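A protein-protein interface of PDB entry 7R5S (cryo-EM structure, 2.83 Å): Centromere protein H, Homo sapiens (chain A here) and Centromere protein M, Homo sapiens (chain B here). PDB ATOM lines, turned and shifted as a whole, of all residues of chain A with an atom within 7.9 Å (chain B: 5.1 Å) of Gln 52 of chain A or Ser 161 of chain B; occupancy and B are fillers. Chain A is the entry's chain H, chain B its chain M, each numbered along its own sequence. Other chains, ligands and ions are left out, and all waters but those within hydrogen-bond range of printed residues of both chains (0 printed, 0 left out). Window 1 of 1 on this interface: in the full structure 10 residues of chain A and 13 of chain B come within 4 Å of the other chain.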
ATOM      1  N   LEU A  46     -10.487   7.976  -9.896  1.00  0.00           N
ATOM      2  CA  LEU A  46     -10.748   9.309 -10.426  1.00  0.00           C
ATOM      3  C   LEU A  46     -12.092   9.840  -9.947  1.00  0.00           C
ATOM      4  O   LEU A  46     -12.203  11.011  -9.568  1.00  0.00           O
ATOM      5  CB  LEU A  46     -10.695   9.285 -11.954  1.00  0.00           C
ATOM      6  CG  LEU A  46     -11.026  10.599 -12.664  1.00  0.00           C
ATOM      7  CD1 LEU A  46     -10.007  11.671 -12.313  1.00  0.00           C
ATOM      8  CD2 LEU A  46     -11.098  10.393 -14.169  1.00  0.00           C
ATOM      9  N   ARG A  47     -13.123   8.992  -9.947  1.00  0.00           N
ATOM     10  CA  ARG A  47     -14.434   9.425  -9.472  1.00  0.00           C
ATOM     11  C   ARG A  47     -14.409   9.721  -7.977  1.00  0.00           C
ATOM     12  O   ARG A  47     -15.006  10.708  -7.523  1.00  0.00           O
ATOM     13  CB  ARG A  47     -15.482   8.361  -9.797  1.00  0.00           C
ATOM     14  CG  ARG A  47     -16.913   8.774  -9.491  1.00  0.00           C
ATOM     15  CD  ARG A  47     -17.430   8.097  -8.232  1.00  0.00           C
ATOM     16  NE  ARG A  47     -17.476   6.644  -8.369  1.00  0.00           N
ATOM     17  CZ  ARG A  47     -18.523   5.971  -8.835  1.00  0.00           C
ATOM     18  NH1 ARG A  47     -19.616   6.620  -9.210  1.00  0.00           N
ATOM     19  NH2 ARG A  47     -18.477   4.649  -8.923  1.00  0.00           N
ATOM     20  N   ALA A  48     -13.722   8.880  -7.197  1.00  0.00           N
ATOM     21  CA  ALA A  48     -13.638   9.106  -5.759  1.00  0.00           C
ATOM     22  C   ALA A  48     -12.928  10.413  -5.436  1.00  0.00           C
ATOM     23  O   ALA A  48     -13.298  11.098  -4.476  1.00  0.00           O
ATOM     24  CB  ALA A  48     -12.927   7.934  -5.083  1.00  0.00           C
ATOM     25  N   GLN A  49     -11.911  10.777  -6.219  1.00  0.00           N
ATOM     26  CA  GLN A  49     -11.234  12.050  -5.985  1.00  0.00           C
ATOM     27  C   GLN A  49     -12.062  13.228  -6.489  1.00  0.00           C
ATOM     28  O   GLN A  49     -12.095  14.290  -5.850  1.00  0.00           O
ATOM     29  CB  GLN A  49      -9.857  12.041  -6.647  1.00  0.00           C
ATOM     30  CG  GLN A  49      -8.889  11.036  -6.046  1.00  0.00           C
ATOM     31  CD  GLN A  49      -7.559  11.004  -6.769  1.00  0.00           C
ATOM     32  OE1 GLN A  49      -7.351  11.729  -7.741  1.00  0.00           O
ATOM     33  NE2 GLN A  49      -6.648  10.163  -6.297  1.00  0.00           N
ATOM     34  N   THR A  50     -12.743  13.057  -7.625  1.00  0.00           N
ATOM     35  CA  THR A  50     -13.517  14.148  -8.203  1.00  0.00           C
ATOM     36  C   THR A  50     -14.705  14.511  -7.324  1.00  0.00           C
ATOM     37  O   THR A  50     -15.053  15.690  -7.204  1.00  0.00           O
ATOM     38  CB  THR A  50     -13.984  13.771  -9.609  1.00  0.00           C
ATOM     39  OG1 THR A  50     -12.864  13.322 -10.380  1.00  0.00           O
ATOM     40  CG2 THR A  50     -14.614  14.969 -10.301  1.00  0.00           C
ATOM     41  N   LYS A  51     -15.340  13.516  -6.701  1.00  0.00           N
ATOM     42  CA  LYS A  51     -16.443  13.810  -5.790  1.00  0.00           C
ATOM     43  C   LYS A  51     -15.970  14.658  -4.614  1.00  0.00           C
ATOM     44  O   LYS A  51     -16.601  15.663  -4.260  1.00  0.00           O
ATOM     45  CB  LYS A  51     -17.076  12.509  -5.296  1.00  0.00           C
ATOM     46  CG  LYS A  51     -18.055  11.885  -6.275  1.00  0.00           C
ATOM     47  CD  LYS A  51     -18.834  10.753  -5.629  1.00  0.00           C
ATOM     48  CE  LYS A  51     -19.954  10.268  -6.533  1.00  0.00           C
ATOM     49  NZ  LYS A  51     -20.741   9.173  -5.904  1.00  0.00           N
ATOM     50  N   GLN A  52     -14.849  14.268  -4.002  1.00  0.00           N
ATOM     51  CA  GLN A  52     -14.322  15.007  -2.862  1.00  0.00           C
ATOM     52  C   GLN A  52     -13.879  16.412  -3.253  1.00  0.00           C
ATOM     53  O   GLN A  52     -14.015  17.346  -2.453  1.00  0.00           O
ATOM     54  CB  GLN A  52     -13.157  14.239  -2.234  1.00  0.00           C
ATOM     55  CG  GLN A  52     -12.609  14.857  -0.957  1.00  0.00           C
ATOM     56  CD  GLN A  52     -13.583  14.770   0.201  1.00  0.00           C
ATOM     57  OE1 GLN A  52     -14.457  13.904   0.229  1.00  0.00           O
ATOM     58  NE2 GLN A  52     -13.436  15.671   1.165  1.00  0.00           N
ATOM     59  N   GLN A  53     -13.357  16.587  -4.469  1.00  0.00           N
ATOM     60  CA  GLN A  53     -12.950  17.924  -4.892  1.00  0.00           C
ATOM     61  C   GLN A  53     -14.153  18.803  -5.224  1.00  0.00           C
ATOM     62  O   GLN A  53     -14.169  19.993  -4.876  1.00  0.00           O
ATOM     63  CB  GLN A  53     -12.004  17.828  -6.087  1.00  0.00           C
ATOM     64  CG  GLN A  53     -10.658  17.206  -5.744  1.00  0.00           C
ATOM     65  CD  GLN A  53      -9.882  16.768  -6.969  1.00  0.00           C
ATOM     66  OE1 GLN A  53     -10.386  16.827  -8.090  1.00  0.00           O
ATOM     67  NE2 GLN A  53      -8.650  16.323  -6.760  1.00  0.00           N
ATOM     68  N   LEU A  54     -15.170  18.240  -5.880  1.00  0.00           N
ATOM     69  CA  LEU A  54     -16.373  18.996  -6.200  1.00  0.00           C
ATOM     70  C   LEU A  54     -17.141  19.395  -4.950  1.00  0.00           C
ATOM     71  O   LEU A  54     -17.729  20.482  -4.914  1.00  0.00           O
ATOM     72  CB  LEU A  54     -17.272  18.180  -7.131  1.00  0.00           C
ATOM     73  CG  LEU A  54     -18.557  18.854  -7.616  1.00  0.00           C
ATOM     74  CD1 LEU A  54     -18.242  20.154  -8.336  1.00  0.00           C
ATOM     75  CD2 LEU A  54     -19.343  17.917  -8.517  1.00  0.00           C
ATOM     76  N   LEU A  55     -17.151  18.540  -3.924  1.00  0.00           N
ATOM     77  CA  LEU A  55     -17.790  18.915  -2.667  1.00  0.00           C
ATOM     78  C   LEU A  55     -17.137  20.156  -2.070  1.00  0.00           C
ATOM     79  O   LEU A  55     -17.830  21.087  -1.642  1.00  0.00           O
ATOM     80  CB  LEU A  55     -17.736  17.748  -1.681  1.00  0.00           C
ATOM     81  CG  LEU A  55     -18.488  17.920  -0.358  1.00  0.00           C
ATOM     82  CD1 LEU A  55     -19.260  16.657  -0.021  1.00  0.00           C
ATOM     83  CD2 LEU A  55     -17.530  18.278   0.769  1.00  0.00           C
ATOM     84  N   GLU A  56     -15.803  20.191  -2.047  1.00  0.00           N
ATOM     85  CA  GLU A  56     -15.098  21.352  -1.514  1.00  0.00           C
ATOM     86  C   GLU A  56     -15.346  22.591  -2.365  1.00  0.00           C
ATOM     87  O   GLU A  56     -15.524  23.692  -1.829  1.00  0.00           O
ATOM     88  CB  GLU A  56     -13.601  21.060  -1.418  1.00  0.00           C
ATOM     89  CG  GLU A  56     -12.793  22.169  -0.766  1.00  0.00           C
ATOM     90  CD  GLU A  56     -11.299  21.925  -0.840  1.00  0.00           C
ATOM     91  OE1 GLU A  56     -10.865  21.144  -1.713  1.00  0.00           O
ATOM     92  OE2 GLU A  56     -10.558  22.513  -0.025  1.00  0.00           O
ATOM     93  N   TYR A  57     -15.358  22.434  -3.692  1.00  0.00           N
ATOM     94  CA  TYR A  57     -15.630  23.573  -4.566  1.00  0.00           C
ATOM     95  C   TYR A  57     -17.015  24.154  -4.296  1.00  0.00           C
ATOM     96  O   TYR A  57     -17.179  25.376  -4.165  1.00  0.00           O
ATOM     97  CB  TYR A  57     -15.499  23.154  -6.030  1.00  0.00           C
ATOM     98  CG  TYR A  57     -14.282  23.717  -6.724  1.00  0.00           C
ATOM     99  CD1 TYR A  57     -14.210  25.061  -7.060  1.00  0.00           C
ATOM    100  CD2 TYR A  57     -13.207  22.902  -7.053  1.00  0.00           C
ATOM    101  CE1 TYR A  57     -13.100  25.580  -7.696  1.00  0.00           C
ATOM    102  CE2 TYR A  57     -12.093  23.412  -7.690  1.00  0.00           C
ATOM    103  CZ  TYR A  57     -12.046  24.751  -8.010  1.00  0.00           C
ATOM    104  OH  TYR A  57     -10.939  25.264  -8.644  1.00  0.00           O
ATOM    105  N   LYS A  58     -18.026  23.286  -4.211  1.00  0.00           N
ATOM    106  CA  LYS A  58     -19.386  23.753  -3.963  1.00  0.00           C
ATOM    107  C   LYS A  58     -19.508  24.394  -2.588  1.00  0.00           C
ATOM    108  O   LYS A  58     -20.201  25.405  -2.427  1.00  0.00           O
ATOM    109  CB  LYS A  58     -20.374  22.596  -4.107  1.00  0.00           C
ATOM    110  CG  LYS A  58     -20.727  22.259  -5.544  1.00  0.00           C
ATOM    111  CD  LYS A  58     -21.903  21.301  -5.609  1.00  0.00           C
ATOM    112  CE  LYS A  58     -22.370  21.098  -7.041  1.00  0.00           C
ATOM    113  NZ  LYS A  58     -23.556  20.202  -7.114  1.00  0.00           N
ATOM    114  N   SER A  59     -18.834  23.827  -1.583  1.00  0.00           N
ATOM    115  CA  SER A  59     -18.877  24.417  -0.249  1.00  0.00           C
ATOM    116  C   SER A  59     -18.239  25.801  -0.238  1.00  0.00           C
ATOM    117  O   SER A  59     -18.762  26.728   0.391  1.00  0.00           O
ATOM    118  CB  SER A  59     -18.183  23.498   0.755  1.00  0.00           C
ATOM    119  OG  SER A  59     -17.784  24.216   1.910  1.00  0.00           O
ATOM    120  N   MET A  60     -17.114  25.963  -0.940  1.00  0.00           N
ATOM    121  CA  MET A  60     -16.468  27.271  -1.003  1.00  0.00           C
ATOM    122  C   MET A  60     -17.350  28.289  -1.713  1.00  0.00           C
ATOM    123  O   MET A  60     -17.465  29.438  -1.266  1.00  0.00           O
ATOM    124  CB  MET A  60     -15.113  27.158  -1.702  1.00  0.00           C
ATOM    125  CG  MET A  60     -14.046  26.443  -0.889  1.00  0.00           C
ATOM    126  SD  MET A  60     -13.573  27.339   0.602  1.00  0.00           S
ATOM    127  CE  MET A  60     -14.363  26.340   1.861  1.00  0.00           C
ATOM    128  N   LYS A  93     -22.052  12.530   8.811  1.00  0.00           N
ATOM    129  CA  LYS A  93     -21.094  11.762   8.025  1.00  0.00           C
ATOM    130  C   LYS A  93     -21.070  10.301   8.456  1.00  0.00           C
ATOM    131  O   LYS A  93     -20.979   9.398   7.613  1.00  0.00           O
ATOM    132  CB  LYS A  93     -19.705  12.384   8.150  1.00  0.00           C
ATOM    133  CG  LYS A  93     -18.696  11.878   7.136  1.00  0.00           C
ATOM    134  CD  LYS A  93     -17.341  12.533   7.344  1.00  0.00           C
ATOM    135  CE  LYS A  93     -17.455  14.048   7.358  1.00  0.00           C
ATOM    136  NZ  LYS A  93     -16.151  14.700   7.654  1.00  0.00           N
ATOM    137  N   ILE B 152      -3.720  14.439   2.606  1.00  0.00           N
ATOM    138  CA  ILE B 152      -5.018  14.763   3.194  1.00  0.00           C
ATOM    139  C   ILE B 152      -5.560  16.063   2.610  1.00  0.00           C
ATOM    140  O   ILE B 152      -6.740  16.159   2.255  1.00  0.00           O
ATOM    141  CB  ILE B 152      -4.913  14.834   4.728  1.00  0.00           C
ATOM    142  CG1 ILE B 152      -4.735  13.434   5.317  1.00  0.00           C
ATOM    143  CG2 ILE B 152      -6.142  15.507   5.318  1.00  0.00           C
ATOM    144  CD1 ILE B 152      -4.714  13.408   6.829  1.00  0.00           C
ATOM    145  N   GLY B 155      -7.095  16.249  -1.175  1.00  0.00           N
ATOM    146  CA  GLY B 155      -8.371  15.645  -1.498  1.00  0.00           C
ATOM    147  C   GLY B 155      -8.309  14.200  -1.927  1.00  0.00           C
ATOM    148  O   GLY B 155      -9.225  13.735  -2.615  1.00  0.00           O
ATOM    149  N   VAL B 157      -8.207  11.652   0.238  1.00  0.00           N
ATOM    150  CA  VAL B 157      -8.758  10.830   1.311  1.00  0.00           C
ATOM    151  C   VAL B 157     -10.260  11.080   1.385  1.00  0.00           C
ATOM    152  O   VAL B 157     -10.685  12.177   1.777  1.00  0.00           O
ATOM    153  CB  VAL B 157      -8.076  11.129   2.656  1.00  0.00           C
ATOM    154  CG1 VAL B 157      -8.689  10.284   3.760  1.00  0.00           C
ATOM    155  CG2 VAL B 157      -6.580  10.879   2.557  1.00  0.00           C
ATOM    156  N   PRO B 158     -11.095  10.108   1.019  1.00  0.00           N
ATOM    157  CA  PRO B 158     -12.547  10.336   1.029  1.00  0.00           C
ATOM    158  C   PRO B 158     -13.068  10.521   2.447  1.00  0.00           C
ATOM    159  O   PRO B 158     -12.843   9.682   3.322  1.00  0.00           O
ATOM    160  CB  PRO B 158     -13.113   9.065   0.382  1.00  0.00           C
ATOM    161  CG  PRO B 158     -11.954   8.443  -0.339  1.00  0.00           C
ATOM    162  CD  PRO B 158     -10.747   8.787   0.472  1.00  0.00           C
ATOM    163  N   GLY B 159     -13.774  11.629   2.666  1.00  0.00           N
ATOM    164  CA  GLY B 159     -14.383  11.924   3.943  1.00  0.00           C
ATOM    165  C   GLY B 159     -13.624  12.910   4.805  1.00  0.00           C
ATOM    166  O   GLY B 159     -14.190  13.410   5.785  1.00  0.00           O
ATOM    167  N   VAL B 160     -12.369  13.206   4.476  1.00  0.00           N
ATOM    168  CA  VAL B 160     -11.540  14.125   5.248  1.00  0.00           C
ATOM    169  C   VAL B 160     -11.037  15.217   4.316  1.00  0.00           C
ATOM    170  O   VAL B 160     -10.485  14.925   3.249  1.00  0.00           O
ATOM    171  CB  VAL B 160     -10.362  13.398   5.924  1.00  0.00           C
ATOM    172  CG1 VAL B 160      -9.536  14.376   6.743  1.00  0.00           C
ATOM    173  CG2 VAL B 160     -10.867  12.260   6.795  1.00  0.00           C
ATOM    174  N   SER B 161     -11.228  16.468   4.719  1.00  0.00           N
ATOM    175  CA  SER B 161     -10.788  17.632   3.964  1.00  0.00           C
ATOM    176  C   SER B 161      -9.883  18.495   4.838  1.00  0.00           C
ATOM    177  O   SER B 161      -9.585  18.160   5.987  1.00  0.00           O
ATOM    178  CB  SER B 161     -11.988  18.434   3.454  1.00  0.00           C
ATOM    179  OG  SER B 161     -12.597  19.165   4.503  1.00  0.00           O
ATOM    180  N   ALA B 162      -9.442  19.624   4.277  1.00  0.00           N
ATOM    181  CA  ALA B 162      -8.585  20.534   5.028  1.00  0.00           C
ATOM    182  C   ALA B 162      -9.348  21.200   6.166  1.00  0.00           C
ATOM    183  O   ALA B 162      -8.784  21.452   7.238  1.00  0.00           O
ATOM    184  CB  ALA B 162      -7.987  21.585   4.094  1.00  0.00           C
ATOM    185  N   LEU B 163     -10.634  21.491   5.953  1.00  0.00           N
ATOM    186  CA  LEU B 163     -11.440  22.089   7.011  1.00  0.00           C
ATOM    187  C   LEU B 163     -11.616  21.136   8.185  1.00  0.00           C
ATOM    188  O   LEU B 163     -11.737  21.580   9.333  1.00  0.00           O
ATOM    189  CB  LEU B 163     -12.800  22.512   6.455  1.00  0.00           C
ATOM    190  CG  LEU B 163     -13.611  23.496   7.297  1.00  0.00           C
ATOM    191  CD1 LEU B 163     -12.810  24.760   7.564  1.00  0.00           C
ATOM    192  CD2 LEU B 163     -14.923  23.828   6.611  1.00  0.00           C
ATOM    193  N   ASN B 164     -11.632  19.828   7.923  1.00  0.00           N
ATOM    194  CA  ASN B 164     -11.681  18.851   9.004  1.00  0.00           C
ATOM    195  C   ASN B 164     -10.329  18.725   9.695  1.00  0.00           C
ATOM    196  O   ASN B 164     -10.264  18.587  10.922  1.00  0.00           O
ATOM    197  CB  ASN B 164     -12.135  17.494   8.463  1.00  0.00           C
ATOM    198  CG  ASN B 164     -12.705  16.594   9.542  1.00  0.00           C
ATOM    199  OD1 ASN B 164     -12.436  16.776  10.728  1.00  0.00           O
ATOM    200  ND2 ASN B 164     -13.500  15.613   9.130  1.00  0.00           N
ATOM    201  N   LEU B 165      -9.241  18.770   8.921  1.00  0.00           N
ATOM    202  CA  LEU B 165      -7.908  18.757   9.512  1.00  0.00           C
ATOM    203  C   LEU B 165      -7.684  19.969  10.404  1.00  0.00           C
ATOM    204  O   LEU B 165      -6.913  19.899  11.367  1.00  0.00           O
ATOM    205  CB  LEU B 165      -6.849  18.698   8.411  1.00  0.00           C
ATOM    206  CG  LEU B 165      -5.396  18.513   8.847  1.00  0.00           C
ATOM    207  CD1 LEU B 165      -5.218  17.187   9.569  1.00  0.00           C
ATOM    208  CD2 LEU B 165      -4.465  18.605   7.650  1.00  0.00           C
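The backbone carbonyl oxygen (O) of Gly 159 of chain B lies within hydrogen-bond range of the side-chain amino group (NZ) of Lys 93 of chain A (3.0 Å). N of Gly 159 of chain B sits at hydrogen-bond distance from OE1 of Gln 52 of chain A, 3.4 Å away. NZ of Lys 93 of chain A lies close to ND2 of Asn 164 of chain B, 3.2 Å away.
The side-chain hydroxyl of Ser 161 of chain B lies close to the backbone NH of Leu 163 of chain B, 3.4 Å away.
Among the printed residues, merely in contact across the chains: Gln 52 of chain A with Val 160 of chain B, Gln 52 of chain A with Ser 161 of chain B and Gln 52 of chain A with Gly 155 of chain B.
Printed residues of chain B within 4 Å of Gln 52 of chain A: Gly 155, Gly 159, Val 160 and Ser 161. Of chain A, only Gln 52 comes within 4 Å of Ser 161 of chain B. No residue of chain A comes within 4 Å of Ala 162 of chain B. Of the printed residues of chain B, Lys 93 of chain A touches Gly 159 and Asn 164. Printed residues of chain A within 4 Å of Asn 164 of chain B: Lys 93. Printed residues of chain A within 4 Å of Val 160 of chain B: Gln 52 (3.7 Å). Printed residues of chain A within 4 Å of Gly 155 of chain B: Gln 52. Of the printed residues of chain A, Gly 159 of chain B touches Gln 52 and Lys 93. The nearest residue of chain B that does not touch Gln 52 of chain A is Pro 158 of chain B (4.1 Å). The nearest residue of chain A that does not touch Ser 161 of chain B is Glu 56 of chain A (5.5 Å). The nearest printed residue of chain A that does not touch Asn 164 of chain B is Gln 52 of chain A (7.6 Å).
Of the 16 printed residues of chain A, 2 touch a printed residue of chain B. Of the 11 printed residues of chain B, 5 touch a printed residue of chain A. Along chain B the printed residues that touch a printed residue of chain A span positions 155 to 164.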
